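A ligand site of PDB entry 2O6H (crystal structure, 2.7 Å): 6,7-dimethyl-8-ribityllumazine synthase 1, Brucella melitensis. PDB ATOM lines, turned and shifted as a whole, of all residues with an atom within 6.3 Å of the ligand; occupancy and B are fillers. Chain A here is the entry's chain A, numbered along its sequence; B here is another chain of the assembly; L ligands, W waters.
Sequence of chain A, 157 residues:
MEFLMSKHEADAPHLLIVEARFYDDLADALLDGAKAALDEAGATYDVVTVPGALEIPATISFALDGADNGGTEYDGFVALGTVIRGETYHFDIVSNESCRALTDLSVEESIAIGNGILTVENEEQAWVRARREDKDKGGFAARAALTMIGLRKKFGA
An oxygen (O8) of the ligand is in hydrogen-bond range of the side-chain carboxylate (OE1) of Glu 55, 2.6 Å away.
The backbone carbonyl oxygen (O) of Thr 82 lies within hydrogen-bond range of a nitrogen (N2) of the ligand, at 2.7 Å.
An oxygen (O1) of the ligand is in hydrogen-bond range of the backbone NH of Ala 53 (2.7 Å).
N of Asn 115 of chain B lies close to O8 of the ligand (3.2 Å).
The backbone carbonyl oxygen (O) of Asn 115 of chain B is in hydrogen-bond range of an oxygen (O7) of the ligand (2.9 Å).
ND1 of His 90 sits close to O4 of the ligand (3.1 Å).
An oxygen (O5) of the ligand sits at hydrogen-bond distance from the backbone NH (N) of Leu 54.
OE2 of Glu 55 sits at hydrogen-bond distance from N of Gly 52, 3.0 Å away.
Ala 20 touches the ligand (CB to O1, 3.8 Å).
Phe 22 touches the ligand.
Tyr 23 touches the ligand.
C of Pro 51 touches O6 of the ligand, at 3.8 Å.
Gly 52 touches the ligand.
Val 83 touches the ligand (CA to O2, 3.0 Å).
Ile 84 touches the ligand (N to O2, 3.8 Å).
CG2 of Val 94 touches C5 of the ligand (3.6 Å).
Phe 140 of chain B touches the ligand (CE2 to O6, 3.3 Å).
Hydrophobic or aromatic side chains within 4 Å of the ligand: Ala 20, Phe 22, Tyr 23, Ala 53, Leu 54, Val 83, His 90, Val 94 and Phe 140 of chain B.
Within 4 Å of the ligand: Ala 20, Phe 22, Tyr 23, Pro 51, Gly 52, Ala 53, Leu 54, Glu 55, Thr 82, Val 83, Ile 84, His 90, Val 94, Asn 115 of chain B and Phe 140 of chain B.
Water W1 lies within hydrogen-bond range of O1 of the ligand, N of Thr 82 and O of Ala 20.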
ATOM      1  N   ALA A  20     -21.802  16.905  32.945  1.00  0.00           N
ATOM      2  CA  ALA A  20     -21.986  16.148  31.730  1.00  0.00           C
ATOM      3  C   ALA A  20     -22.769  17.126  30.856  1.00  0.00           C
ATOM      4  O   ALA A  20     -23.926  17.434  31.150  1.00  0.00           O
ATOM      5  CB  ALA A  20     -22.789  14.901  32.014  1.00  0.00           C
ATOM      6  N   ARG A  21     -22.116  17.643  29.829  1.00  0.00           N
ATOM      7  CA  ARG A  21     -22.717  18.616  28.928  1.00  0.00           C
ATOM      8  C   ARG A  21     -23.128  17.949  27.615  1.00  0.00           C
ATOM      9  O   ARG A  21     -22.355  17.903  26.656  1.00  0.00           O
ATOM     10  CB  ARG A  21     -21.734  19.751  28.677  1.00  0.00           C
ATOM     11  CG  ARG A  21     -22.258  20.892  27.855  1.00  0.00           C
ATOM     12  CD  ARG A  21     -21.251  22.029  27.902  1.00  0.00           C
ATOM     13  NE  ARG A  21     -21.324  22.748  29.170  1.00  0.00           N
ATOM     14  CZ  ARG A  21     -22.200  23.713  29.443  1.00  0.00           C
ATOM     15  NH1 ARG A  21     -23.093  24.095  28.534  1.00  0.00           N
ATOM     16  NH2 ARG A  21     -22.211  24.285  30.631  1.00  0.00           N
ATOM     17  N   PHE A  22     -24.353  17.430  27.601  1.00  0.00           N
ATOM     18  CA  PHE A  22     -24.893  16.763  26.441  1.00  0.00           C
ATOM     19  C   PHE A  22     -25.873  17.722  25.792  1.00  0.00           C
ATOM     20  O   PHE A  22     -25.928  17.832  24.589  1.00  0.00           O
ATOM     21  CB  PHE A  22     -25.620  15.492  26.856  1.00  0.00           C
ATOM     22  CG  PHE A  22     -25.917  14.566  25.713  1.00  0.00           C
ATOM     23  CD1 PHE A  22     -24.898  13.820  25.138  1.00  0.00           C
ATOM     24  CD2 PHE A  22     -27.210  14.439  25.220  1.00  0.00           C
ATOM     25  CE1 PHE A  22     -25.163  12.954  24.078  1.00  0.00           C
ATOM     26  CE2 PHE A  22     -27.486  13.578  24.169  1.00  0.00           C
ATOM     27  CZ  PHE A  22     -26.466  12.824  23.600  1.00  0.00           C
ATOM     28  N   TYR A  23     -26.676  18.404  26.610  1.00  0.00           N
ATOM     29  CA  TYR A  23     -27.636  19.385  26.126  1.00  0.00           C
ATOM     30  C   TYR A  23     -27.078  20.717  26.598  1.00  0.00           C
ATOM     31  O   TYR A  23     -27.354  21.161  27.717  1.00  0.00           O
ATOM     32  CB  TYR A  23     -29.008  19.152  26.742  1.00  0.00           C
ATOM     33  CG  TYR A  23     -29.614  17.816  26.371  1.00  0.00           C
ATOM     34  CD1 TYR A  23     -29.564  16.738  27.257  1.00  0.00           C
ATOM     35  CD2 TYR A  23     -30.221  17.628  25.141  1.00  0.00           C
ATOM     36  CE1 TYR A  23     -30.105  15.504  26.915  1.00  0.00           C
ATOM     37  CE2 TYR A  23     -30.773  16.401  24.779  1.00  0.00           C
ATOM     38  CZ  TYR A  23     -30.717  15.351  25.682  1.00  0.00           C
ATOM     39  OH  TYR A  23     -31.270  14.128  25.342  1.00  0.00           O
ATOM     40  N   PRO A  51     -18.379  14.699  28.297  1.00  0.00           N
ATOM     41  CA  PRO A  51     -19.398  14.579  27.250  1.00  0.00           C
ATOM     42  C   PRO A  51     -20.741  14.013  27.647  1.00  0.00           C
ATOM     43  O   PRO A  51     -21.755  14.359  27.037  1.00  0.00           O
ATOM     44  CB  PRO A  51     -18.694  13.734  26.191  1.00  0.00           C
ATOM     45  CG  PRO A  51     -17.845  12.847  26.987  1.00  0.00           C
ATOM     46  CD  PRO A  51     -17.264  13.762  28.042  1.00  0.00           C
ATOM     47  N   GLY A  52     -20.771  13.134  28.648  1.00  0.00           N
ATOM     48  CA  GLY A  52     -22.039  12.542  29.061  1.00  0.00           C
ATOM     49  C   GLY A  52     -22.069  12.028  30.489  1.00  0.00           C
ATOM     50  O   GLY A  52     -21.028  11.842  31.128  1.00  0.00           O
ATOM     51  N   ALA A  53     -23.279  11.789  30.986  1.00  0.00           N
ATOM     52  CA  ALA A  53     -23.457  11.309  32.358  1.00  0.00           C
ATOM     53  C   ALA A  53     -22.715  10.017  32.604  1.00  0.00           C
ATOM     54  O   ALA A  53     -22.405   9.701  33.743  1.00  0.00           O
ATOM     55  CB  ALA A  53     -24.942  11.125  32.676  1.00  0.00           C
ATOM     56  N   LEU A  54     -22.411   9.269  31.539  1.00  0.00           N
ATOM     57  CA  LEU A  54     -21.696   8.015  31.726  1.00  0.00           C
ATOM     58  C   LEU A  54     -20.280   8.262  32.212  1.00  0.00           C
ATOM     59  O   LEU A  54     -19.747   7.450  32.989  1.00  0.00           O
ATOM     60  CB  LEU A  54     -21.693   7.163  30.453  1.00  0.00           C
ATOM     61  CG  LEU A  54     -23.037   6.470  30.141  1.00  0.00           C
ATOM     62  CD1 LEU A  54     -22.882   5.555  28.935  1.00  0.00           C
ATOM     63  CD2 LEU A  54     -23.500   5.660  31.347  1.00  0.00           C
ATOM     64  N   GLU A  55     -19.647   9.354  31.790  1.00  0.00           N
ATOM     65  CA  GLU A  55     -18.292   9.599  32.271  1.00  0.00           C
ATOM     66  C   GLU A  55     -18.182  10.447  33.547  1.00  0.00           C
ATOM     67  O   GLU A  55     -17.088  10.804  33.947  1.00  0.00           O
ATOM     68  CB  GLU A  55     -17.384  10.228  31.183  1.00  0.00           C
ATOM     69  CG  GLU A  55     -18.070  10.951  30.060  1.00  0.00           C
ATOM     70  CD  GLU A  55     -18.606  10.006  29.022  1.00  0.00           C
ATOM     71  OE1 GLU A  55     -18.198   8.824  29.027  1.00  0.00           O
ATOM     72  OE2 GLU A  55     -19.434  10.433  28.187  1.00  0.00           O
ATOM     73  N   ILE A  56     -19.301  10.738  34.193  1.00  0.00           N
ATOM     74  CA  ILE A  56     -19.226  11.535  35.415  1.00  0.00           C
ATOM     75  C   ILE A  56     -18.518  10.806  36.558  1.00  0.00           C
ATOM     76  O   ILE A  56     -17.555  11.306  37.126  1.00  0.00           O
ATOM     77  CB  ILE A  56     -20.634  11.979  35.894  1.00  0.00           C
ATOM     78  CG1 ILE A  56     -21.237  12.956  34.886  1.00  0.00           C
ATOM     79  CG2 ILE A  56     -20.542  12.619  37.270  1.00  0.00           C
ATOM     80  CD1 ILE A  56     -22.615  13.451  35.262  1.00  0.00           C
ATOM     81  N   GLY A  81     -26.007  16.704  35.321  1.00  0.00           N
ATOM     82  CA  GLY A  81     -26.249  16.059  34.048  1.00  0.00           C
ATOM     83  C   GLY A  81     -27.725  16.010  33.704  1.00  0.00           C
ATOM     84  O   GLY A  81     -28.578  16.368  34.520  1.00  0.00           O
ATOM     85  N   THR A  82     -28.058  15.566  32.504  1.00  0.00           N
ATOM     86  CA  THR A  82     -29.450  15.499  32.120  1.00  0.00           C
ATOM     87  C   THR A  82     -29.702  14.482  31.017  1.00  0.00           C
ATOM     88  O   THR A  82     -29.016  14.465  29.999  1.00  0.00           O
ATOM     89  CB  THR A  82     -29.956  16.883  31.684  1.00  0.00           C
ATOM     90  OG1 THR A  82     -29.887  17.777  32.802  1.00  0.00           O
ATOM     91  CG2 THR A  82     -31.399  16.806  31.187  1.00  0.00           C
ATOM     92  N   VAL A  83     -30.688  13.621  31.252  1.00  0.00           N
ATOM     93  CA  VAL A  83     -31.065  12.577  30.299  1.00  0.00           C
ATOM     94  C   VAL A  83     -32.575  12.697  30.073  1.00  0.00           C
ATOM     95  O   VAL A  83     -33.372  12.571  31.002  1.00  0.00           O
ATOM     96  CB  VAL A  83     -30.753  11.151  30.837  1.00  0.00           C
ATOM     97  CG1 VAL A  83     -30.776  10.151  29.707  1.00  0.00           C
ATOM     98  CG2 VAL A  83     -29.392  11.125  31.525  1.00  0.00           C
ATOM     99  N   ILE A  84     -32.948  12.957  28.831  1.00  0.00           N
ATOM    100  CA  ILE A  84     -34.351  13.089  28.453  1.00  0.00           C
ATOM    101  C   ILE A  84     -34.718  11.807  27.717  1.00  0.00           C
ATOM    102  O   ILE A  84     -34.024  11.423  26.776  1.00  0.00           O
ATOM    103  CB  ILE A  84     -34.541  14.276  27.475  1.00  0.00           C
ATOM    104  CG1 ILE A  84     -33.846  15.513  28.026  1.00  0.00           C
ATOM    105  CG2 ILE A  84     -36.022  14.536  27.269  1.00  0.00           C
ATOM    106  CD1 ILE A  84     -33.805  16.649  27.064  1.00  0.00           C
ATOM    107  N   HIS A  90     -31.730   3.610  25.435  1.00  0.00           N
ATOM    108  CA  HIS A  90     -30.480   4.262  25.796  1.00  0.00           C
ATOM    109  C   HIS A  90     -30.693   5.159  27.008  1.00  0.00           C
ATOM    110  O   HIS A  90     -29.812   5.301  27.856  1.00  0.00           O
ATOM    111  CB  HIS A  90     -29.939   5.093  24.633  1.00  0.00           C
ATOM    112  CG  HIS A  90     -28.512   5.499  24.786  1.00  0.00           C
ATOM    113  ND1 HIS A  90     -28.090   6.802  24.647  1.00  0.00           N
ATOM    114  CD2 HIS A  90     -27.412   4.768  25.085  1.00  0.00           C
ATOM    115  CE1 HIS A  90     -26.781   6.861  24.848  1.00  0.00           C
ATOM    116  NE2 HIS A  90     -26.353   5.640  25.118  1.00  0.00           N
ATOM    117  N   PHE A  91     -31.872   5.775  27.077  1.00  0.00           N
ATOM    118  CA  PHE A  91     -32.222   6.633  28.191  1.00  0.00           C
ATOM    119  C   PHE A  91     -32.034   5.878  29.503  1.00  0.00           C
ATOM    120  O   PHE A  91     -31.287   6.297  30.382  1.00  0.00           O
ATOM    121  CB  PHE A  91     -33.680   7.075  28.073  1.00  0.00           C
ATOM    122  CG  PHE A  91     -34.222   7.686  29.338  1.00  0.00           C
ATOM    123  CD1 PHE A  91     -33.895   8.995  29.686  1.00  0.00           C
ATOM    124  CD2 PHE A  91     -35.013   6.933  30.204  1.00  0.00           C
ATOM    125  CE1 PHE A  91     -34.349   9.554  30.886  1.00  0.00           C
ATOM    126  CE2 PHE A  91     -35.475   7.483  31.410  1.00  0.00           C
ATOM    127  CZ  PHE A  91     -35.149   8.794  31.745  1.00  0.00           C
ATOM    128  N   VAL A  94     -28.182   5.064  30.186  1.00  0.00           N
ATOM    129  CA  VAL A  94     -27.428   6.238  30.600  1.00  0.00           C
ATOM    130  C   VAL A  94     -27.836   6.713  31.989  1.00  0.00           C
ATOM    131  O   VAL A  94     -26.992   7.090  32.797  1.00  0.00           O
ATOM    132  CB  VAL A  94     -27.604   7.401  29.605  1.00  0.00           C
ATOM    133  CG1 VAL A  94     -26.965   8.674  30.147  1.00  0.00           C
ATOM    134  CG2 VAL A  94     -26.958   7.028  28.290  1.00  0.00           C
ATOM    135  N   ILE B 113     -12.752   5.517  29.021  1.00  0.00           N
ATOM    136  CA  ILE B 113     -13.573   4.667  28.158  1.00  0.00           C
ATOM    137  C   ILE B 113     -14.655   5.423  27.377  1.00  0.00           C
ATOM    138  O   ILE B 113     -15.423   6.186  27.954  1.00  0.00           O
ATOM    139  CB  ILE B 113     -14.300   3.564  28.965  1.00  0.00           C
ATOM    140  CG1 ILE B 113     -13.295   2.637  29.617  1.00  0.00           C
ATOM    141  CG2 ILE B 113     -15.223   2.776  28.054  1.00  0.00           C
ATOM    142  CD1 ILE B 113     -13.963   1.549  30.431  1.00  0.00           C
ATOM    143  N   GLY B 114     -14.726   5.174  26.075  1.00  0.00           N
ATOM    144  CA  GLY B 114     -15.748   5.807  25.259  1.00  0.00           C
ATOM    145  C   GLY B 114     -16.824   4.766  25.025  1.00  0.00           C
ATOM    146  O   GLY B 114     -16.573   3.749  24.389  1.00  0.00           O
ATOM    147  N   ASN B 115     -18.028   5.008  25.533  1.00  0.00           N
ATOM    148  CA  ASN B 115     -19.125   4.046  25.400  1.00  0.00           C
ATOM    149  C   ASN B 115     -19.910   4.219  24.104  1.00  0.00           C
ATOM    150  O   ASN B 115     -20.733   5.132  23.986  1.00  0.00           O
ATOM    151  CB  ASN B 115     -20.076   4.156  26.584  1.00  0.00           C
ATOM    152  CG  ASN B 115     -20.947   2.943  26.717  1.00  0.00           C
ATOM    153  OD1 ASN B 115     -21.311   2.324  25.706  1.00  0.00           O
ATOM    154  ND2 ASN B 115     -21.310   2.592  27.951  1.00  0.00           N
ATOM    155  N   GLY B 116     -19.683   3.319  23.140  1.00  0.00           N
ATOM    156  CA  GLY B 116     -20.361   3.391  21.860  1.00  0.00           C
ATOM    157  C   GLY B 116     -21.276   2.223  21.565  1.00  0.00           C
ATOM    158  O   GLY B 116     -21.468   1.854  20.410  1.00  0.00           O
ATOM    159  N   LYS B 137     -22.385   8.241  16.377  1.00  0.00           N
ATOM    160  CA  LYS B 137     -22.117   7.824  17.735  1.00  0.00           C
ATOM    161  C   LYS B 137     -20.730   7.184  17.863  1.00  0.00           C
ATOM    162  O   LYS B 137     -20.054   7.362  18.877  1.00  0.00           O
ATOM    163  CB  LYS B 137     -23.194   6.858  18.226  1.00  0.00           C
ATOM    164  CG  LYS B 137     -24.557   7.498  18.346  1.00  0.00           C
ATOM    165  CD  LYS B 137     -24.471   8.829  19.088  1.00  0.00           C
ATOM    166  CE  LYS B 137     -25.800   9.562  19.123  1.00  0.00           C
ATOM    167  NZ  LYS B 137     -25.678  10.917  19.760  1.00  0.00           N
ATOM    168  N   PHE B 140     -18.476   9.894  18.187  1.00  0.00           N
ATOM    169  CA  PHE B 140     -18.803  10.547  19.442  1.00  0.00           C
ATOM    170  C   PHE B 140     -18.110   9.788  20.568  1.00  0.00           C
ATOM    171  O   PHE B 140     -17.483  10.391  21.441  1.00  0.00           O
ATOM    172  CB  PHE B 140     -20.317  10.541  19.665  1.00  0.00           C
ATOM    173  CG  PHE B 140     -20.760  11.355  20.855  1.00  0.00           C
ATOM    174  CD1 PHE B 140     -20.939  12.749  20.744  1.00  0.00           C
ATOM    175  CD2 PHE B 140     -21.021  10.746  22.089  1.00  0.00           C
ATOM    176  CE1 PHE B 140     -21.376  13.508  21.850  1.00  0.00           C
ATOM    177  CE2 PHE B 140     -21.458  11.505  23.195  1.00  0.00           C
ATOM    178  CZ  PHE B 140     -21.634  12.879  23.074  1.00  0.00           C
ATOM    179  N   ALA B 141     -18.217   8.457  20.545  1.00  0.00           N
ATOM    180  CA  ALA B 141     -17.593   7.606  21.557  1.00  0.00           C
ATOM    181  C   ALA B 141     -16.062   7.726  21.579  1.00  0.00           C
ATOM    182  O   ALA B 141     -15.441   7.739  22.642  1.00  0.00           O
ATOM    183  CB  ALA B 141     -17.996   6.150  21.331  1.00  0.00           C
ATOM    184  N   ALA B 144     -14.968  10.850  23.180  1.00  0.00           N
ATOM    185  CA  ALA B 144     -15.176  10.760  24.621  1.00  0.00           C
ATOM    186  C   ALA B 144     -13.919  10.162  25.255  1.00  0.00           C
ATOM    187  O   ALA B 144     -13.381  10.704  26.231  1.00  0.00           O
ATOM    188  CB  ALA B 144     -16.390   9.880  24.911  1.00  0.00           C
ATOM    189  N   ALA B 145     -13.470   9.053  24.690  1.00  0.00           N
ATOM    190  CA  ALA B 145     -12.272   8.362  25.160  1.00  0.00           C
ATOM    191  C   ALA B 145     -11.122   9.354  25.146  1.00  0.00           C
ATOM    192  O   ALA B 145     -10.348   9.416  26.110  1.00  0.00           O
ATOM    193  CB  ALA B 145     -11.947   7.170  24.249  1.00  0.00           C
HETATM  194  N1  LIG L   1     -25.311  11.812  28.035  1.00  0.00           N
HETATM  195  C1  LIG L   1     -26.032  12.568  28.958  1.00  0.00           C
HETATM  196  O1  LIG L   1     -25.387  13.123  29.832  1.00  0.00           O
HETATM  197  N2  LIG L   1     -27.400  12.626  28.785  1.00  0.00           N
HETATM  198  C2  LIG L   1     -28.115  11.988  27.776  1.00  0.00           C
HETATM  199  O2  LIG L   1     -29.371  12.190  27.834  1.00  0.00           O
HETATM  200  C3  LIG L   1     -27.287  11.125  26.733  1.00  0.00           C
HETATM  201  N3  LIG L   1     -28.038  10.451  25.672  1.00  0.00           N
HETATM  202  O3  LIG L   1     -29.219  10.550  25.590  1.00  0.00           O
HETATM  203  O4  LIG L   1     -27.440   9.787  24.855  1.00  0.00           O
HETATM  204  C4  LIG L   1     -25.809  11.079  26.946  1.00  0.00           C
HETATM  205  N4  LIG L   1     -24.813  10.395  26.165  1.00  0.00           N
HETATM  206  C5  LIG L   1     -24.470   9.023  26.650  1.00  0.00           C
HETATM  207  C6  LIG L   1     -23.123   8.906  27.486  1.00  0.00           C
HETATM  208  O5  LIG L   1     -23.320   9.871  28.492  1.00  0.00           O
HETATM  209  C7  LIG L   1     -21.732   9.334  26.832  1.00  0.00           C
HETATM  210  O6  LIG L   1     -21.829  10.618  26.317  1.00  0.00           O
HETATM  211  C8  LIG L   1     -21.048   8.399  25.574  1.00  0.00           C
HETATM  212  O7  LIG L   1     -22.031   7.299  25.486  1.00  0.00           O
HETATM  213  C9  LIG L   1     -19.698   7.538  25.631  1.00  0.00           C
HETATM  214  O8  LIG L   1     -19.142   7.728  26.906  1.00  0.00           O
HETATM  215  O   HOH W   1     -26.168  15.349  30.711  1.00  0.00           O
